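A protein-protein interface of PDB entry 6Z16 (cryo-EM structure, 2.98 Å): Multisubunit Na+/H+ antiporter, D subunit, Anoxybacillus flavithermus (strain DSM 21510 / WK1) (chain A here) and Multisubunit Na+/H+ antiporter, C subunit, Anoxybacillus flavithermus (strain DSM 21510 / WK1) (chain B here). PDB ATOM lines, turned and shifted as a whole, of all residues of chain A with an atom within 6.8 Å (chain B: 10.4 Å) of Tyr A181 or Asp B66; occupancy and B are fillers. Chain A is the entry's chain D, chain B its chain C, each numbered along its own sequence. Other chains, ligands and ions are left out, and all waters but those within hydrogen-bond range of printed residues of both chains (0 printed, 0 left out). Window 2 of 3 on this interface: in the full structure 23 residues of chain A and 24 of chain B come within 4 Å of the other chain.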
ATOM      1  N   ALA A 176     -31.775  24.191   8.079  1.00  0.00           N
ATOM      2  CA  ALA A 176     -32.088  22.847   7.591  1.00  0.00           C
ATOM      3  C   ALA A 176     -30.890  22.207   6.895  1.00  0.00           C
ATOM      4  O   ALA A 176     -30.611  21.013   7.097  1.00  0.00           O
ATOM      5  CB  ALA A 176     -33.289  22.905   6.653  1.00  0.00           C
ATOM      6  N   VAL A 177     -30.173  22.988   6.077  1.00  0.00           N
ATOM      7  CA  VAL A 177     -28.948  22.505   5.437  1.00  0.00           C
ATOM      8  C   VAL A 177     -27.897  22.152   6.486  1.00  0.00           C
ATOM      9  O   VAL A 177     -27.187  21.146   6.356  1.00  0.00           O
ATOM     10  CB  VAL A 177     -28.439  23.555   4.425  1.00  0.00           C
ATOM     11  CG1 VAL A 177     -27.053  23.227   3.914  1.00  0.00           C
ATOM     12  CG2 VAL A 177     -29.381  23.634   3.251  1.00  0.00           C
ATOM     13  N   ALA A 178     -27.836  22.931   7.574  1.00  0.00           N
ATOM     14  CA  ALA A 178     -26.883  22.661   8.653  1.00  0.00           C
ATOM     15  C   ALA A 178     -27.174  21.339   9.358  1.00  0.00           C
ATOM     16  O   ALA A 178     -26.262  20.531   9.584  1.00  0.00           O
ATOM     17  CB  ALA A 178     -26.902  23.808   9.658  1.00  0.00           C
ATOM     18  N   TYR A 179     -28.445  21.108   9.709  1.00  0.00           N
ATOM     19  CA  TYR A 179     -28.852  19.848  10.335  1.00  0.00           C
ATOM     20  C   TYR A 179     -28.571  18.652   9.435  1.00  0.00           C
ATOM     21  O   TYR A 179     -28.039  17.626   9.889  1.00  0.00           O
ATOM     22  CB  TYR A 179     -30.338  19.885  10.650  1.00  0.00           C
ATOM     23  CG  TYR A 179     -30.797  20.855  11.704  1.00  0.00           C
ATOM     24  CD1 TYR A 179     -29.946  21.314  12.690  1.00  0.00           C
ATOM     25  CD2 TYR A 179     -32.092  21.343  11.679  1.00  0.00           C
ATOM     26  CE1 TYR A 179     -30.387  22.215  13.642  1.00  0.00           C
ATOM     27  CE2 TYR A 179     -32.535  22.241  12.615  1.00  0.00           C
ATOM     28  CZ  TYR A 179     -31.682  22.672  13.595  1.00  0.00           C
ATOM     29  OH  TYR A 179     -32.133  23.569  14.530  1.00  0.00           O
ATOM     30  N   LEU A 180     -28.915  18.767   8.150  1.00  0.00           N
ATOM     31  CA  LEU A 180     -28.733  17.639   7.246  1.00  0.00           C
ATOM     32  C   LEU A 180     -27.258  17.388   6.949  1.00  0.00           C
ATOM     33  O   LEU A 180     -26.864  16.238   6.722  1.00  0.00           O
ATOM     34  CB  LEU A 180     -29.533  17.873   5.965  1.00  0.00           C
ATOM     35  CG  LEU A 180     -29.624  16.729   4.957  1.00  0.00           C
ATOM     36  CD1 LEU A 180     -30.241  15.502   5.592  1.00  0.00           C
ATOM     37  CD2 LEU A 180     -30.457  17.175   3.796  1.00  0.00           C
ATOM     38  N   TYR A 181     -26.425  18.434   6.983  1.00  0.00           N
ATOM     39  CA  TYR A 181     -24.990  18.226   6.830  1.00  0.00           C
ATOM     40  C   TYR A 181     -24.404  17.543   8.053  1.00  0.00           C
ATOM     41  O   TYR A 181     -23.478  16.734   7.935  1.00  0.00           O
ATOM     42  CB  TYR A 181     -24.268  19.549   6.574  1.00  0.00           C
ATOM     43  CG  TYR A 181     -22.777  19.368   6.394  1.00  0.00           C
ATOM     44  CD1 TYR A 181     -22.263  18.814   5.230  1.00  0.00           C
ATOM     45  CD2 TYR A 181     -21.884  19.733   7.393  1.00  0.00           C
ATOM     46  CE1 TYR A 181     -20.906  18.634   5.063  1.00  0.00           C
ATOM     47  CE2 TYR A 181     -20.525  19.551   7.235  1.00  0.00           C
ATOM     48  CZ  TYR A 181     -20.044  19.001   6.067  1.00  0.00           C
ATOM     49  OH  TYR A 181     -18.692  18.824   5.899  1.00  0.00           O
ATOM     50  N   ALA A 182     -24.927  17.860   9.238  1.00  0.00           N
ATOM     51  CA  ALA A 182     -24.449  17.176  10.432  1.00  0.00           C
ATOM     52  C   ALA A 182     -24.854  15.712  10.455  1.00  0.00           C
ATOM     53  O   ALA A 182     -24.126  14.882  11.006  1.00  0.00           O
ATOM     54  CB  ALA A 182     -24.967  17.864  11.676  1.00  0.00           C
ATOM     55  N   VAL A 183     -26.004  15.375   9.875  1.00  0.00           N
ATOM     56  CA  VAL A 183     -26.399  13.969   9.830  1.00  0.00           C
ATOM     57  C   VAL A 183     -25.621  13.212   8.757  1.00  0.00           C
ATOM     58  O   VAL A 183     -25.022  12.166   9.030  1.00  0.00           O
ATOM     59  CB  VAL A 183     -27.915  13.837   9.615  1.00  0.00           C
ATOM     60  CG1 VAL A 183     -28.285  12.386   9.506  1.00  0.00           C
ATOM     61  CG2 VAL A 183     -28.659  14.478  10.751  1.00  0.00           C
ATOM     62  N   THR A 184     -25.607  13.728   7.527  1.00  0.00           N
ATOM     63  CA  THR A 184     -25.098  13.001   6.364  1.00  0.00           C
ATOM     64  C   THR A 184     -23.640  13.298   6.040  1.00  0.00           C
ATOM     65  O   THR A 184     -22.840  12.373   5.887  1.00  0.00           O
ATOM     66  CB  THR A 184     -25.967  13.315   5.142  1.00  0.00           C
ATOM     67  OG1 THR A 184     -26.067  14.735   4.984  1.00  0.00           O
ATOM     68  CG2 THR A 184     -27.347  12.721   5.298  1.00  0.00           C
ATOM     69  N   GLY A 185     -23.279  14.568   5.911  1.00  0.00           N
ATOM     70  CA  GLY A 185     -21.918  14.942   5.608  1.00  0.00           C
ATOM     71  C   GLY A 185     -21.650  15.358   4.178  1.00  0.00           C
ATOM     72  O   GLY A 185     -20.513  15.720   3.868  1.00  0.00           O
ATOM     73  N   THR A 186     -22.644  15.319   3.300  1.00  0.00           N
ATOM     74  CA  THR A 186     -22.495  15.718   1.907  1.00  0.00           C
ATOM     75  C   THR A 186     -23.488  16.815   1.569  1.00  0.00           C
ATOM     76  O   THR A 186     -24.287  17.245   2.400  1.00  0.00           O
ATOM     77  CB  THR A 186     -22.691  14.536   0.961  1.00  0.00           C
ATOM     78  OG1 THR A 186     -23.960  13.937   1.214  1.00  0.00           O
ATOM     79  CG2 THR A 186     -21.635  13.527   1.174  1.00  0.00           C
ATOM     80  N   LEU A 187     -23.424  17.272   0.325  1.00  0.00           N
ATOM     81  CA  LEU A 187     -24.227  18.413  -0.079  1.00  0.00           C
ATOM     82  C   LEU A 187     -24.880  18.263  -1.452  1.00  0.00           C
ATOM     83  O   LEU A 187     -25.814  19.014  -1.743  1.00  0.00           O
ATOM     84  CB  LEU A 187     -23.353  19.677  -0.034  1.00  0.00           C
ATOM     85  CG  LEU A 187     -23.959  21.076  -0.009  1.00  0.00           C
ATOM     86  CD1 LEU A 187     -24.852  21.231   1.203  1.00  0.00           C
ATOM     87  CD2 LEU A 187     -22.846  22.090   0.052  1.00  0.00           C
ATOM     88  N   LEU B  42     -24.819  28.275  13.849  1.00  0.00           N
ATOM     89  CA  LEU B  42     -25.314  26.907  13.807  1.00  0.00           C
ATOM     90  C   LEU B  42     -24.645  26.104  12.699  1.00  0.00           C
ATOM     91  O   LEU B  42     -24.346  24.923  12.890  1.00  0.00           O
ATOM     92  CB  LEU B  42     -26.830  26.905  13.644  1.00  0.00           C
ATOM     93  CG  LEU B  42     -27.488  25.530  13.689  1.00  0.00           C
ATOM     94  CD1 LEU B  42     -27.206  24.859  15.005  1.00  0.00           C
ATOM     95  CD2 LEU B  42     -28.964  25.676  13.501  1.00  0.00           C
ATOM     96  N   LEU B  43     -24.404  26.726  11.536  1.00  0.00           N
ATOM     97  CA  LEU B  43     -23.620  26.066  10.488  1.00  0.00           C
ATOM     98  C   LEU B  43     -22.225  25.700  10.973  1.00  0.00           C
ATOM     99  O   LEU B  43     -21.759  24.571  10.750  1.00  0.00           O
ATOM    100  CB  LEU B  43     -23.510  26.951   9.252  1.00  0.00           C
ATOM    101  CG  LEU B  43     -24.611  27.050   8.209  1.00  0.00           C
ATOM    102  CD1 LEU B  43     -24.313  28.204   7.285  1.00  0.00           C
ATOM    103  CD2 LEU B  43     -24.629  25.763   7.416  1.00  0.00           C
ATOM    104  N   LEU B  44     -21.562  26.634  11.670  1.00  0.00           N
ATOM    105  CA  LEU B  44     -20.222  26.364  12.187  1.00  0.00           C
ATOM    106  C   LEU B  44     -20.232  25.261  13.240  1.00  0.00           C
ATOM    107  O   LEU B  44     -19.347  24.398  13.250  1.00  0.00           O
ATOM    108  CB  LEU B  44     -19.614  27.636  12.772  1.00  0.00           C
ATOM    109  CG  LEU B  44     -18.150  27.515  13.188  1.00  0.00           C
ATOM    110  CD1 LEU B  44     -17.292  27.174  11.986  1.00  0.00           C
ATOM    111  CD2 LEU B  44     -17.689  28.800  13.829  1.00  0.00           C
ATOM    112  N   THR B  45     -21.238  25.260  14.117  1.00  0.00           N
ATOM    113  CA  THR B  45     -21.307  24.275  15.191  1.00  0.00           C
ATOM    114  C   THR B  45     -21.599  22.884  14.649  1.00  0.00           C
ATOM    115  O   THR B  45     -20.944  21.909  15.032  1.00  0.00           O
ATOM    116  CB  THR B  45     -22.375  24.686  16.203  1.00  0.00           C
ATOM    117  OG1 THR B  45     -22.086  25.997  16.696  1.00  0.00           O
ATOM    118  CG2 THR B  45     -22.403  23.716  17.363  1.00  0.00           C
ATOM    119  N   MET B  46     -22.567  22.770  13.736  1.00  0.00           N
ATOM    120  CA  MET B  46     -22.938  21.462  13.215  1.00  0.00           C
ATOM    121  C   MET B  46     -21.916  20.921  12.230  1.00  0.00           C
ATOM    122  O   MET B  46     -21.911  19.715  11.969  1.00  0.00           O
ATOM    123  CB  MET B  46     -24.321  21.523  12.562  1.00  0.00           C
ATOM    124  CG  MET B  46     -25.415  21.988  13.512  1.00  0.00           C
ATOM    125  SD  MET B  46     -25.702  20.981  14.963  1.00  0.00           S
ATOM    126  CE  MET B  46     -26.713  19.704  14.259  1.00  0.00           C
ATOM    127  N   GLY B  47     -21.044  21.777  11.689  1.00  0.00           N
ATOM    128  CA  GLY B  47     -19.889  21.265  10.972  1.00  0.00           C
ATOM    129  C   GLY B  47     -18.913  20.514  11.857  1.00  0.00           C
ATOM    130  O   GLY B  47     -18.229  19.598  11.393  1.00  0.00           O
ATOM    131  N   GLY B  48     -18.841  20.876  13.136  1.00  0.00           N
ATOM    132  CA  GLY B  48     -17.906  20.262  14.060  1.00  0.00           C
ATOM    133  C   GLY B  48     -16.976  21.288  14.671  1.00  0.00           C
ATOM    134  O   GLY B  48     -16.626  22.272  14.014  1.00  0.00           O
ATOM    135  N   LEU B  49     -16.570  21.085  15.927  1.00  0.00           N
ATOM    136  CA  LEU B  49     -15.708  22.041  16.614  1.00  0.00           C
ATOM    137  C   LEU B  49     -14.489  21.375  17.246  1.00  0.00           C
ATOM    138  O   LEU B  49     -13.896  21.939  18.168  1.00  0.00           O
ATOM    139  CB  LEU B  49     -16.492  22.813  17.679  1.00  0.00           C
ATOM    140  CG  LEU B  49     -17.639  23.697  17.189  1.00  0.00           C
ATOM    141  CD1 LEU B  49     -18.367  24.327  18.355  1.00  0.00           C
ATOM    142  CD2 LEU B  49     -17.155  24.756  16.227  1.00  0.00           C
ATOM    143  N   LYS B  50     -14.104  20.193  16.775  1.00  0.00           N
ATOM    144  CA  LYS B  50     -12.947  19.502  17.332  1.00  0.00           C
ATOM    145  C   LYS B  50     -11.662  20.199  16.896  1.00  0.00           C
ATOM    146  O   LYS B  50     -11.564  20.706  15.778  1.00  0.00           O
ATOM    147  CB  LYS B  50     -12.958  18.037  16.893  1.00  0.00           C
ATOM    148  CG  LYS B  50     -11.866  17.162  17.494  1.00  0.00           C
ATOM    149  CD  LYS B  50     -11.982  17.069  19.006  1.00  0.00           C
ATOM    150  CE  LYS B  50     -13.214  16.287  19.423  1.00  0.00           C
ATOM    151  NZ  LYS B  50     -13.093  14.841  19.102  1.00  0.00           N
ATOM    152  N   ALA B  51     -10.672  20.221  17.790  1.00  0.00           N
ATOM    153  CA  ALA B  51      -9.517  21.100  17.633  1.00  0.00           C
ATOM    154  C   ALA B  51      -8.547  20.606  16.562  1.00  0.00           C
ATOM    155  O   ALA B  51      -8.144  19.438  16.553  1.00  0.00           O
ATOM    156  CB  ALA B  51      -8.788  21.244  18.965  1.00  0.00           C
ATOM    157  N   GLY B  52      -8.168  21.516  15.674  1.00  0.00           N
ATOM    158  CA  GLY B  52      -7.138  21.297  14.687  1.00  0.00           C
ATOM    159  C   GLY B  52      -6.634  22.629  14.176  1.00  0.00           C
ATOM    160  O   GLY B  52      -6.973  23.686  14.709  1.00  0.00           O
ATOM    161  N   ALA B  53      -5.829  22.567  13.125  1.00  0.00           N
ATOM    162  CA  ALA B  53      -5.238  23.763  12.550  1.00  0.00           C
ATOM    163  C   ALA B  53      -6.270  24.555  11.753  1.00  0.00           C
ATOM    164  O   ALA B  53      -7.290  24.008  11.337  1.00  0.00           O
ATOM    165  CB  ALA B  53      -4.073  23.379  11.649  1.00  0.00           C
ATOM    166  N   PRO B  54      -6.036  25.853  11.551  1.00  0.00           N
ATOM    167  CA  PRO B  54      -6.848  26.600  10.596  1.00  0.00           C
ATOM    168  C   PRO B  54      -6.677  26.042   9.197  1.00  0.00           C
ATOM    169  O   PRO B  54      -5.637  25.440   8.876  1.00  0.00           O
ATOM    170  CB  PRO B  54      -6.294  28.027  10.707  1.00  0.00           C
ATOM    171  CG  PRO B  54      -5.784  28.105  12.070  1.00  0.00           C
ATOM    172  CD  PRO B  54      -5.215  26.758  12.374  1.00  0.00           C
ATOM    173  N   PRO B  55      -7.694  26.198   8.329  1.00  0.00           N
ATOM    174  CA  PRO B  55      -7.650  25.520   7.026  1.00  0.00           C
ATOM    175  C   PRO B  55      -6.643  26.127   6.061  1.00  0.00           C
ATOM    176  O   PRO B  55      -7.006  26.859   5.138  1.00  0.00           O
ATOM    177  CB  PRO B  55      -9.084  25.672   6.513  1.00  0.00           C
ATOM    178  CG  PRO B  55      -9.585  26.883   7.177  1.00  0.00           C
ATOM    179  CD  PRO B  55      -8.964  26.916   8.527  1.00  0.00           C
ATOM    180  N   LEU B  56      -5.364  25.825   6.281  1.00  0.00           N
ATOM    181  CA  LEU B  56      -4.266  26.393   5.509  1.00  0.00           C
ATOM    182  C   LEU B  56      -3.205  25.316   5.379  1.00  0.00           C
ATOM    183  O   LEU B  56      -2.699  24.832   6.393  1.00  0.00           O
ATOM    184  CB  LEU B  56      -3.684  27.626   6.202  1.00  0.00           C
ATOM    185  CG  LEU B  56      -4.544  28.870   6.431  1.00  0.00           C
ATOM    186  CD1 LEU B  56      -3.812  29.858   7.302  1.00  0.00           C
ATOM    187  CD2 LEU B  56      -4.930  29.504   5.124  1.00  0.00           C
ATOM    188  N   ARG B  63      -4.173  17.072  11.452  1.00  0.00           N
ATOM    189  CA  ARG B  63      -5.585  17.179  11.125  1.00  0.00           C
ATOM    190  C   ARG B  63      -6.003  18.640  11.123  1.00  0.00           C
ATOM    191  O   ARG B  63      -5.458  19.464  11.860  1.00  0.00           O
ATOM    192  CB  ARG B  63      -6.459  16.373  12.094  1.00  0.00           C
ATOM    193  CG  ARG B  63      -6.368  16.808  13.536  1.00  0.00           C
ATOM    194  CD  ARG B  63      -7.268  15.971  14.415  1.00  0.00           C
ATOM    195  NE  ARG B  63      -8.676  16.194  14.106  1.00  0.00           N
ATOM    196  CZ  ARG B  63      -9.667  15.426  14.543  1.00  0.00           C
ATOM    197  NH1 ARG B  63     -10.918  15.704  14.210  1.00  0.00           N
ATOM    198  NH2 ARG B  63      -9.406  14.383  15.317  1.00  0.00           N
ATOM    199  N   TYR B  64      -6.979  18.948  10.278  1.00  0.00           N
ATOM    200  CA  TYR B  64      -7.445  20.303  10.049  1.00  0.00           C
ATOM    201  C   TYR B  64      -8.906  20.432  10.456  1.00  0.00           C
ATOM    202  O   TYR B  64      -9.639  19.447  10.535  1.00  0.00           O
ATOM    203  CB  TYR B  64      -7.296  20.690   8.574  1.00  0.00           C
ATOM    204  CG  TYR B  64      -5.873  20.797   8.091  1.00  0.00           C
ATOM    205  CD1 TYR B  64      -5.156  21.978   8.231  1.00  0.00           C
ATOM    206  CD2 TYR B  64      -5.244  19.713   7.500  1.00  0.00           C
ATOM    207  CE1 TYR B  64      -3.859  22.074   7.789  1.00  0.00           C
ATOM    208  CE2 TYR B  64      -3.948  19.800   7.059  1.00  0.00           C
ATOM    209  CZ  TYR B  64      -3.261  20.981   7.207  1.00  0.00           C
ATOM    210  OH  TYR B  64      -1.969  21.059   6.763  1.00  0.00           O
ATOM    211  N   VAL B  65      -9.316  21.671  10.715  1.00  0.00           N
ATOM    212  CA  VAL B  65     -10.728  21.990  10.858  1.00  0.00           C
ATOM    213  C   VAL B  65     -11.401  21.847   9.493  1.00  0.00           C
ATOM    214  O   VAL B  65     -10.767  22.040   8.449  1.00  0.00           O
ATOM    215  CB  VAL B  65     -10.854  23.409  11.453  1.00  0.00           C
ATOM    216  CG1 VAL B  65     -12.293  23.886  11.600  1.00  0.00           C
ATOM    217  CG2 VAL B  65     -10.193  23.444  12.809  1.00  0.00           C
ATOM    218  N   ASP B  66     -12.678  21.442   9.504  1.00  0.00           N
ATOM    219  CA  ASP B  66     -13.460  21.188   8.296  1.00  0.00           C
ATOM    220  C   ASP B  66     -13.554  22.435   7.414  1.00  0.00           C
ATOM    221  O   ASP B  66     -13.968  23.499   7.895  1.00  0.00           O
ATOM    222  CB  ASP B  66     -14.855  20.723   8.716  1.00  0.00           C
ATOM    223  CG  ASP B  66     -15.659  20.109   7.584  1.00  0.00           C
ATOM    224  OD1 ASP B  66     -15.174  20.022   6.444  1.00  0.00           O
ATOM    225  OD2 ASP B  66     -16.813  19.719   7.843  1.00  0.00           O
ATOM    226  N   PRO B  67     -13.164  22.350   6.130  1.00  0.00           N
ATOM    227  CA  PRO B  67     -13.173  23.538   5.265  1.00  0.00           C
ATOM    228  C   PRO B  67     -14.527  23.905   4.669  1.00  0.00           C
ATOM    229  O   PRO B  67     -14.745  25.079   4.359  1.00  0.00           O
ATOM    230  CB  PRO B  67     -12.193  23.155   4.153  1.00  0.00           C
ATOM    231  CG  PRO B  67     -11.386  22.054   4.701  1.00  0.00           C
ATOM    232  CD  PRO B  67     -12.297  21.296   5.583  1.00  0.00           C
ATOM    233  N   LEU B  68     -15.415  22.922   4.465  1.00  0.00           N
ATOM    234  CA  LEU B  68     -16.717  23.194   3.849  1.00  0.00           C
ATOM    235  C   LEU B  68     -17.628  24.153   4.614  1.00  0.00           C
ATOM    236  O   LEU B  68     -18.146  25.088   3.971  1.00  0.00           O
ATOM    237  CB  LEU B  68     -17.464  21.889   3.559  1.00  0.00           C
ATOM    238  CG  LEU B  68     -17.185  21.136   2.280  1.00  0.00           C
ATOM    239  CD1 LEU B  68     -17.903  19.813   2.314  1.00  0.00           C
ATOM    240  CD2 LEU B  68     -17.712  21.984   1.155  1.00  0.00           C
ATOM    241  N   PRO B  69     -17.909  23.984   5.929  1.00  0.00           N
ATOM    242  CA  PRO B  69     -18.891  24.878   6.557  1.00  0.00           C
ATOM    243  C   PRO B  69     -18.443  26.315   6.608  1.00  0.00           C
ATOM    244  O   PRO B  69     -19.293  27.200   6.561  1.00  0.00           O
ATOM    245  CB  PRO B  69     -19.048  24.299   7.968  1.00  0.00           C
ATOM    246  CG  PRO B  69     -18.583  22.938   7.875  1.00  0.00           C
ATOM    247  CD  PRO B  69     -17.461  22.994   6.928  1.00  0.00           C
ATOM    248  N   GLN B  70     -17.139  26.568   6.611  1.00  0.00           N
ATOM    249  CA  GLN B  70     -16.647  27.939   6.608  1.00  0.00           C
ATOM    250  C   GLN B  70     -16.944  28.632   5.281  1.00  0.00           C
ATOM    251  O   GLN B  70     -17.376  29.793   5.262  1.00  0.00           O
ATOM    252  CB  GLN B  70     -15.155  27.934   6.909  1.00  0.00           C
ATOM    253  CG  GLN B  70     -14.826  27.373   8.269  1.00  0.00           C
ATOM    254  CD  GLN B  70     -13.368  27.507   8.606  1.00  0.00           C
ATOM    255  OE1 GLN B  70     -12.593  28.052   7.831  1.00  0.00           O
ATOM    256  NE2 GLN B  70     -12.979  26.997   9.762  1.00  0.00           N
ATOM    257  N   ALA B  71     -16.764  27.917   4.167  1.00  0.00           N
ATOM    258  CA  ALA B  71     -17.105  28.461   2.855  1.00  0.00           C
ATOM    259  C   ALA B  71     -18.607  28.688   2.716  1.00  0.00           C
ATOM    260  O   ALA B  71     -19.040  29.712   2.158  1.00  0.00           O
ATOM    261  CB  ALA B  71     -16.599  27.524   1.763  1.00  0.00           C
ATOM    262  N   LEU B  72     -19.415  27.760   3.248  1.00  0.00           N
ATOM    263  CA  LEU B  72     -20.866  27.931   3.210  1.00  0.00           C
ATOM    264  C   LEU B  72     -21.310  29.128   4.045  1.00  0.00           C
ATOM    265  O   LEU B  72     -22.203  29.884   3.635  1.00  0.00           O
ATOM    266  CB  LEU B  72     -21.559  26.666   3.710  1.00  0.00           C
ATOM    267  CG  LEU B  72     -21.262  25.327   3.037  1.00  0.00           C
ATOM    268  CD1 LEU B  72     -22.009  24.205   3.728  1.00  0.00           C
ATOM    269  CD2 LEU B  72     -21.534  25.343   1.556  1.00  0.00           C
ATOM    270  N   ILE B  73     -20.680  29.321   5.209  1.00  0.00           N
ATOM    271  CA  ILE B  73     -20.972  30.468   6.063  1.00  0.00           C
ATOM    272  C   ILE B  73     -20.613  31.765   5.365  1.00  0.00           C
ATOM    273  O   ILE B  73     -21.363  32.737   5.439  1.00  0.00           O
ATOM    274  CB  ILE B  73     -20.245  30.336   7.416  1.00  0.00           C
ATOM    275  CG1 ILE B  73     -20.904  29.288   8.277  1.00  0.00           C
ATOM    276  CG2 ILE B  73     -20.297  31.608   8.218  1.00  0.00           C
ATOM    277  CD1 ILE B  73     -20.051  28.887   9.398  1.00  0.00           C
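OH of Tyr A181 is in hydrogen-bond range of OD2 of Asp B66 (2.8 Å).
Ala A178 touches Leu B43 (CB to CD2, 3.7 Å).
CB of Met B46 touches O of Ala A178, at 3.7 Å.
Tyr A179 touches Leu B42.
Tyr A179 touches Met B46.
Tyr A181 touches Leu B68 (OH to CD1, 3.8 Å).
Tyr A181 touches Pro B69 (CE2 to CG, 3.96 Å).
Ala A182 touches Met B46.
Leu A187 touches Leu B72.
Of the printed residues of chain A, Asp B66 touches Tyr A181.
No residue of chain B comes within 4 Å of Thr A184.
Printed residues of chain A within 4 Å of Leu B42: Tyr A179 (3.7 Å).
Printed residues of chain A within 4 Å of Leu B68: Tyr A181.
Ala B53 touches none of the printed residues of chain A.
Printed residues of chain B that touch a printed residue of chain A: Leu B42, Leu B43, Met B46, Asp B66, Leu B68, Pro B69 and Leu B72.
Among the printed residues, no Asp or Glu carboxylate lies within 4 Å of a Lys or Arg side-chain nitrogen of the other chain.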
